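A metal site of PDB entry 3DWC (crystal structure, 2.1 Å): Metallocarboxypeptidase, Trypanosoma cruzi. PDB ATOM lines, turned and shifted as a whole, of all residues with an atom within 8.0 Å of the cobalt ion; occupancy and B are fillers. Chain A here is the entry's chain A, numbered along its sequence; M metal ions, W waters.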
ATOM      1  N   PRO A 238     -30.054 -29.415 -27.592  1.00  0.00           N
ATOM      2  CA  PRO A 238     -29.756 -28.030 -27.901  1.00  0.00           C
ATOM      3  C   PRO A 238     -28.644 -27.854 -28.911  1.00  0.00           C
ATOM      4  O   PRO A 238     -27.557 -28.419 -28.735  1.00  0.00           O
ATOM      5  CB  PRO A 238     -29.319 -27.449 -26.561  1.00  0.00           C
ATOM      6  CG  PRO A 238     -30.062 -28.282 -25.553  1.00  0.00           C
ATOM      7  CD  PRO A 238     -30.083 -29.642 -26.137  1.00  0.00           C
ATOM      8  N   PHE A 239     -28.895 -27.045 -29.928  1.00  0.00           N
ATOM      9  CA  PHE A 239     -27.869 -26.732 -30.908  1.00  0.00           C
ATOM     10  C   PHE A 239     -28.102 -25.384 -31.509  1.00  0.00           C
ATOM     11  O   PHE A 239     -29.101 -24.745 -31.270  1.00  0.00           O
ATOM     12  CB  PHE A 239     -27.834 -27.830 -31.999  1.00  0.00           C
ATOM     13  CG  PHE A 239     -29.102 -27.923 -32.833  1.00  0.00           C
ATOM     14  CD1 PHE A 239     -29.213 -27.251 -34.038  1.00  0.00           C
ATOM     15  CD2 PHE A 239     -30.152 -28.739 -32.435  1.00  0.00           C
ATOM     16  CE1 PHE A 239     -30.370 -27.348 -34.822  1.00  0.00           C
ATOM     17  CE2 PHE A 239     -31.312 -28.842 -33.206  1.00  0.00           C
ATOM     18  CZ  PHE A 239     -31.409 -28.129 -34.405  1.00  0.00           C
ATOM     19  N   CYS A 240     -27.143 -24.970 -32.297  1.00  0.00           N
ATOM     20  CA  CYS A 240     -27.188 -23.732 -33.033  1.00  0.00           C
ATOM     21  C   CYS A 240     -27.051 -24.185 -34.485  1.00  0.00           C
ATOM     22  O   CYS A 240     -26.075 -24.865 -34.879  1.00  0.00           O
ATOM     23  CB  CYS A 240     -26.055 -22.803 -32.594  1.00  0.00           C
ATOM     24  SG  CYS A 240     -25.926 -21.289 -33.600  1.00  0.00           S
ATOM     25  N   GLY A 264     -27.392 -22.904 -21.199  1.00  0.00           N
ATOM     26  CA  GLY A 264     -27.427 -23.505 -22.524  1.00  0.00           C
ATOM     27  C   GLY A 264     -27.856 -22.558 -23.632  1.00  0.00           C
ATOM     28  O   GLY A 264     -27.238 -22.523 -24.683  1.00  0.00           O
ATOM     29  N   HIS A 267     -25.122 -19.981 -24.103  1.00  0.00           N
ATOM     30  CA  HIS A 267     -24.066 -20.648 -24.845  1.00  0.00           C
ATOM     31  C   HIS A 267     -24.334 -20.617 -26.358  1.00  0.00           C
ATOM     32  O   HIS A 267     -23.493 -20.233 -27.166  1.00  0.00           O
ATOM     33  CB  HIS A 267     -23.999 -22.134 -24.400  1.00  0.00           C
ATOM     34  CG  HIS A 267     -22.876 -22.917 -25.036  1.00  0.00           C
ATOM     35  ND1 HIS A 267     -21.678 -23.166 -24.397  1.00  0.00           N
ATOM     36  CD2 HIS A 267     -22.790 -23.533 -26.243  1.00  0.00           C
ATOM     37  CE1 HIS A 267     -20.893 -23.854 -25.200  1.00  0.00           C
ATOM     38  NE2 HIS A 267     -21.554 -24.131 -26.306  1.00  0.00           N
ATOM     39  N   GLU A 268     -25.500 -21.089 -26.739  1.00  0.00           N
ATOM     40  CA  GLU A 268     -25.898 -21.166 -28.161  1.00  0.00           C
ATOM     41  C   GLU A 268     -26.063 -19.804 -28.800  1.00  0.00           C
ATOM     42  O   GLU A 268     -25.716 -19.555 -29.969  1.00  0.00           O
ATOM     43  CB  GLU A 268     -27.213 -21.987 -28.249  1.00  0.00           C
ATOM     44  CG  GLU A 268     -27.113 -23.515 -27.868  1.00  0.00           C
ATOM     45  CD  GLU A 268     -25.902 -24.253 -28.481  1.00  0.00           C
ATOM     46  OE1 GLU A 268     -25.487 -23.870 -29.593  1.00  0.00           O
ATOM     47  OE2 GLU A 268     -25.392 -25.240 -27.894  1.00  0.00           O
ATOM     48  N   GLY A 270     -24.194 -17.328 -27.864  1.00  0.00           N
ATOM     49  CA  GLY A 270     -22.818 -16.862 -28.155  1.00  0.00           C
ATOM     50  C   GLY A 270     -22.332 -17.362 -29.520  1.00  0.00           C
ATOM     51  O   GLY A 270     -21.648 -16.655 -30.216  1.00  0.00           O
ATOM     52  N   HIS A 271     -22.661 -18.606 -29.884  1.00  0.00           N
ATOM     53  CA  HIS A 271     -22.431 -19.171 -31.239  1.00  0.00           C
ATOM     54  C   HIS A 271     -23.190 -18.409 -32.309  1.00  0.00           C
ATOM     55  O   HIS A 271     -22.617 -17.966 -33.329  1.00  0.00           O
ATOM     56  CB  HIS A 271     -22.921 -20.617 -31.278  1.00  0.00           C
ATOM     57  CG  HIS A 271     -21.977 -21.634 -30.715  1.00  0.00           C
ATOM     58  ND1 HIS A 271     -20.633 -21.680 -31.048  1.00  0.00           N
ATOM     59  CD2 HIS A 271     -22.204 -22.714 -29.916  1.00  0.00           C
ATOM     60  CE1 HIS A 271     -20.078 -22.737 -30.464  1.00  0.00           C
ATOM     61  NE2 HIS A 271     -21.008 -23.381 -29.780  1.00  0.00           N
ATOM     62  N   LEU A 294     -13.593 -24.656 -34.985  1.00  0.00           N
ATOM     63  CA  LEU A 294     -14.453 -25.028 -33.860  1.00  0.00           C
ATOM     64  C   LEU A 294     -13.941 -24.437 -32.541  1.00  0.00           C
ATOM     65  O   LEU A 294     -14.728 -24.044 -31.640  1.00  0.00           O
ATOM     66  CB  LEU A 294     -14.570 -26.555 -33.775  1.00  0.00           C
ATOM     67  CG  LEU A 294     -15.588 -27.211 -34.681  1.00  0.00           C
ATOM     68  CD1 LEU A 294     -15.602 -28.798 -34.439  1.00  0.00           C
ATOM     69  CD2 LEU A 294     -16.939 -26.738 -34.373  1.00  0.00           C
ATOM     70  N   HIS A 297     -15.057 -20.861 -32.546  1.00  0.00           N
ATOM     71  CA  HIS A 297     -16.526 -20.902 -32.410  1.00  0.00           C
ATOM     72  C   HIS A 297     -16.943 -21.101 -30.987  1.00  0.00           C
ATOM     73  O   HIS A 297     -17.762 -20.366 -30.465  1.00  0.00           O
ATOM     74  CB  HIS A 297     -17.193 -22.016 -33.292  1.00  0.00           C
ATOM     75  CG  HIS A 297     -18.399 -21.530 -34.029  1.00  0.00           C
ATOM     76  ND1 HIS A 297     -19.412 -20.825 -33.404  1.00  0.00           N
ATOM     77  CD2 HIS A 297     -18.690 -21.490 -35.356  1.00  0.00           C
ATOM     78  CE1 HIS A 297     -20.320 -20.472 -34.291  1.00  0.00           C
ATOM     79  NE2 HIS A 297     -19.903 -20.847 -35.483  1.00  0.00           N
ATOM     80  N   GLU A 298     -16.368 -22.143 -30.384  1.00  0.00           N
ATOM     81  CA  GLU A 298     -16.575 -22.466 -28.962  1.00  0.00           C
ATOM     82  C   GLU A 298     -16.010 -21.380 -28.056  1.00  0.00           C
ATOM     83  O   GLU A 298     -16.485 -21.169 -26.942  1.00  0.00           O
ATOM     84  CB  GLU A 298     -15.990 -23.836 -28.645  1.00  0.00           C
ATOM     85  CG  GLU A 298     -16.374 -24.398 -27.273  1.00  0.00           C
ATOM     86  CD  GLU A 298     -17.844 -24.745 -27.139  1.00  0.00           C
ATOM     87  OE1 GLU A 298     -18.187 -25.347 -26.134  1.00  0.00           O
ATOM     88  OE2 GLU A 298     -18.648 -24.467 -28.053  1.00  0.00           O
ATOM     89  N   GLY A 299     -15.038 -20.633 -28.559  1.00  0.00           N
ATOM     90  CA  GLY A 299     -14.597 -19.425 -27.887  1.00  0.00           C
ATOM     91  C   GLY A 299     -15.663 -18.356 -27.730  1.00  0.00           C
ATOM     92  O   GLY A 299     -15.684 -17.590 -26.733  1.00  0.00           O
ATOM     93  N   GLN A 300     -16.520 -18.253 -28.751  1.00  0.00           N
ATOM     94  CA  GLN A 300     -17.619 -17.275 -28.726  1.00  0.00           C
ATOM     95  C   GLN A 300     -18.733 -17.720 -27.814  1.00  0.00           C
ATOM     96  O   GLN A 300     -19.273 -16.925 -27.098  1.00  0.00           O
ATOM     97  CB  GLN A 300     -18.149 -17.004 -30.124  1.00  0.00           C
ATOM     98  CG  GLN A 300     -17.051 -16.578 -31.146  1.00  0.00           C
ATOM     99  CD  GLN A 300     -16.047 -15.659 -30.551  1.00  0.00           C
ATOM    100  OE1 GLN A 300     -16.345 -14.499 -30.224  1.00  0.00           O
ATOM    101  NE2 GLN A 300     -14.802 -16.153 -30.439  1.00  0.00           N
ATOM    102  N   SER A 301     -19.054 -19.003 -27.843  1.00  0.00           N
ATOM    103  CA  SER A 301     -20.072 -19.566 -26.949  1.00  0.00           C
ATOM    104  C   SER A 301     -19.642 -19.520 -25.488  1.00  0.00           C
ATOM    105  O   SER A 301     -20.447 -19.204 -24.598  1.00  0.00           O
ATOM    106  CB  SER A 301     -20.333 -20.969 -27.334  1.00  0.00           C
ATOM    107  OG  SER A 301     -19.087 -21.630 -27.266  1.00  0.00           O
ATOM    108  N   LEU A 302     -18.379 -19.852 -25.226  1.00  0.00           N
ATOM    109  CA  LEU A 302     -17.856 -19.760 -23.869  1.00  0.00           C
ATOM    110  C   LEU A 302     -17.527 -18.378 -23.370  1.00  0.00           C
ATOM    111  O   LEU A 302     -17.524 -18.159 -22.172  1.00  0.00           O
ATOM    112  CB  LEU A 302     -16.668 -20.679 -23.662  1.00  0.00           C
ATOM    113  CG  LEU A 302     -16.977 -22.163 -23.896  1.00  0.00           C
ATOM    114  CD1 LEU A 302     -15.722 -22.987 -23.845  1.00  0.00           C
ATOM    115  CD2 LEU A 302     -18.013 -22.722 -22.907  1.00  0.00           C
ATOM    116  N   GLU A 305     -21.140 -17.737 -22.232  1.00  0.00           N
ATOM    117  CA  GLU A 305     -21.574 -18.551 -21.142  1.00  0.00           C
ATOM    118  C   GLU A 305     -20.701 -18.491 -19.915  1.00  0.00           C
ATOM    119  O   GLU A 305     -21.200 -18.315 -18.790  1.00  0.00           O
ATOM    120  CB  GLU A 305     -21.644 -20.023 -21.543  1.00  0.00           C
ATOM    121  CG  GLU A 305     -22.259 -20.892 -20.466  1.00  0.00           C
ATOM    122  CD  GLU A 305     -21.973 -22.372 -20.669  1.00  0.00           C
ATOM    123  OE1 GLU A 305     -21.459 -22.798 -21.757  1.00  0.00           O
ATOM    124  OE2 GLU A 305     -22.283 -23.085 -19.707  1.00  0.00           O
ATOM    125  N   TYR A 358     -13.988 -29.453 -16.411  1.00  0.00           N
ATOM    126  CA  TYR A 358     -14.208 -29.654 -17.840  1.00  0.00           C
ATOM    127  C   TYR A 358     -12.930 -29.929 -18.672  1.00  0.00           C
ATOM    128  O   TYR A 358     -12.926 -30.883 -19.422  1.00  0.00           O
ATOM    129  CB  TYR A 358     -15.025 -28.512 -18.452  1.00  0.00           C
ATOM    130  CG  TYR A 358     -15.771 -28.948 -19.687  1.00  0.00           C
ATOM    131  CD1 TYR A 358     -17.108 -29.315 -19.628  1.00  0.00           C
ATOM    132  CD2 TYR A 358     -15.118 -29.029 -20.920  1.00  0.00           C
ATOM    133  CE1 TYR A 358     -17.775 -29.761 -20.758  1.00  0.00           C
ATOM    134  CE2 TYR A 358     -15.774 -29.450 -22.051  1.00  0.00           C
ATOM    135  CZ  TYR A 358     -17.101 -29.789 -21.959  1.00  0.00           C
ATOM    136  OH  TYR A 358     -17.748 -30.207 -23.086  1.00  0.00           O
ATOM    137  N   TYR A 419     -12.098 -34.198 -32.507  1.00  0.00           N
ATOM    138  CA  TYR A 419     -13.034 -33.117 -32.223  1.00  0.00           C
ATOM    139  C   TYR A 419     -12.884 -32.560 -30.786  1.00  0.00           C
ATOM    140  O   TYR A 419     -12.840 -31.372 -30.551  1.00  0.00           O
ATOM    141  CB  TYR A 419     -14.427 -33.710 -32.434  1.00  0.00           C
ATOM    142  CG  TYR A 419     -15.577 -32.767 -32.333  1.00  0.00           C
ATOM    143  CD1 TYR A 419     -16.093 -32.390 -31.101  1.00  0.00           C
ATOM    144  CD2 TYR A 419     -16.172 -32.252 -33.473  1.00  0.00           C
ATOM    145  CE1 TYR A 419     -17.154 -31.539 -31.030  1.00  0.00           C
ATOM    146  CE2 TYR A 419     -17.245 -31.411 -33.418  1.00  0.00           C
ATOM    147  CZ  TYR A 419     -17.728 -31.058 -32.184  1.00  0.00           C
ATOM    148  OH  TYR A 419     -18.814 -30.218 -32.124  1.00  0.00           O
ATOM    149  N   TYR A 423     -12.969 -28.124 -27.617  1.00  0.00           N
ATOM    150  CA  TYR A 423     -13.644 -27.602 -26.445  1.00  0.00           C
ATOM    151  C   TYR A 423     -12.745 -26.780 -25.548  1.00  0.00           C
ATOM    152  O   TYR A 423     -13.127 -25.680 -25.178  1.00  0.00           O
ATOM    153  CB  TYR A 423     -14.308 -28.714 -25.605  1.00  0.00           C
ATOM    154  CG  TYR A 423     -15.493 -29.390 -26.254  1.00  0.00           C
ATOM    155  CD1 TYR A 423     -16.737 -28.777 -26.330  1.00  0.00           C
ATOM    156  CD2 TYR A 423     -15.395 -30.678 -26.724  1.00  0.00           C
ATOM    157  CE1 TYR A 423     -17.826 -29.420 -26.937  1.00  0.00           C
ATOM    158  CE2 TYR A 423     -16.458 -31.318 -27.341  1.00  0.00           C
ATOM    159  CZ  TYR A 423     -17.671 -30.690 -27.451  1.00  0.00           C
ATOM    160  OH  TYR A 423     -18.726 -31.411 -28.052  1.00  0.00           O
HETATM  161 CO    CO M   1     -20.869 -25.064 -28.128  1.00  0.00          CO
HETATM  162  O   HOH W   1     -23.029 -26.068 -28.672  1.00  0.00           O
HETATM  163  O   HOH W   2     -20.632 -26.466 -29.973  1.00  0.00           O
HETATM  164  O   HOH W   3     -20.490 -26.983 -26.969  1.00  0.00           O
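The side-chain hydroxyl (OG) of Ser 301 lies within hydrogen-bond range of the backbone carbonyl oxygen (O) of Glu 298 (2.7 Å). The side-chain carboxylate (OE1) of Glu 305 is in hydrogen-bond range of a ring nitrogen (ND1) of His 267, at 2.7 Å. ND1 of His 297 sits at hydrogen-bond distance from ND1 of His 271.
OG of Ser 301 touches the cobalt ion, at 3.96 Å. Within 4 Å of the cobalt ion: His 267, His 271, Glu 298 and Ser 301. Along chain A the residues within 4 Å of the cobalt ion span positions 267 to 301. The nearest printed residue that does not touch the cobalt ion is Glu 268 (4.5 Å).
The cobalt ion is bound by a ring nitrogen (NE2) of His 267, water W3, the side-chain carboxylate (OE2) of Glu 298, water W2, a ring nitrogen (NE2) of His 271 and water W1.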
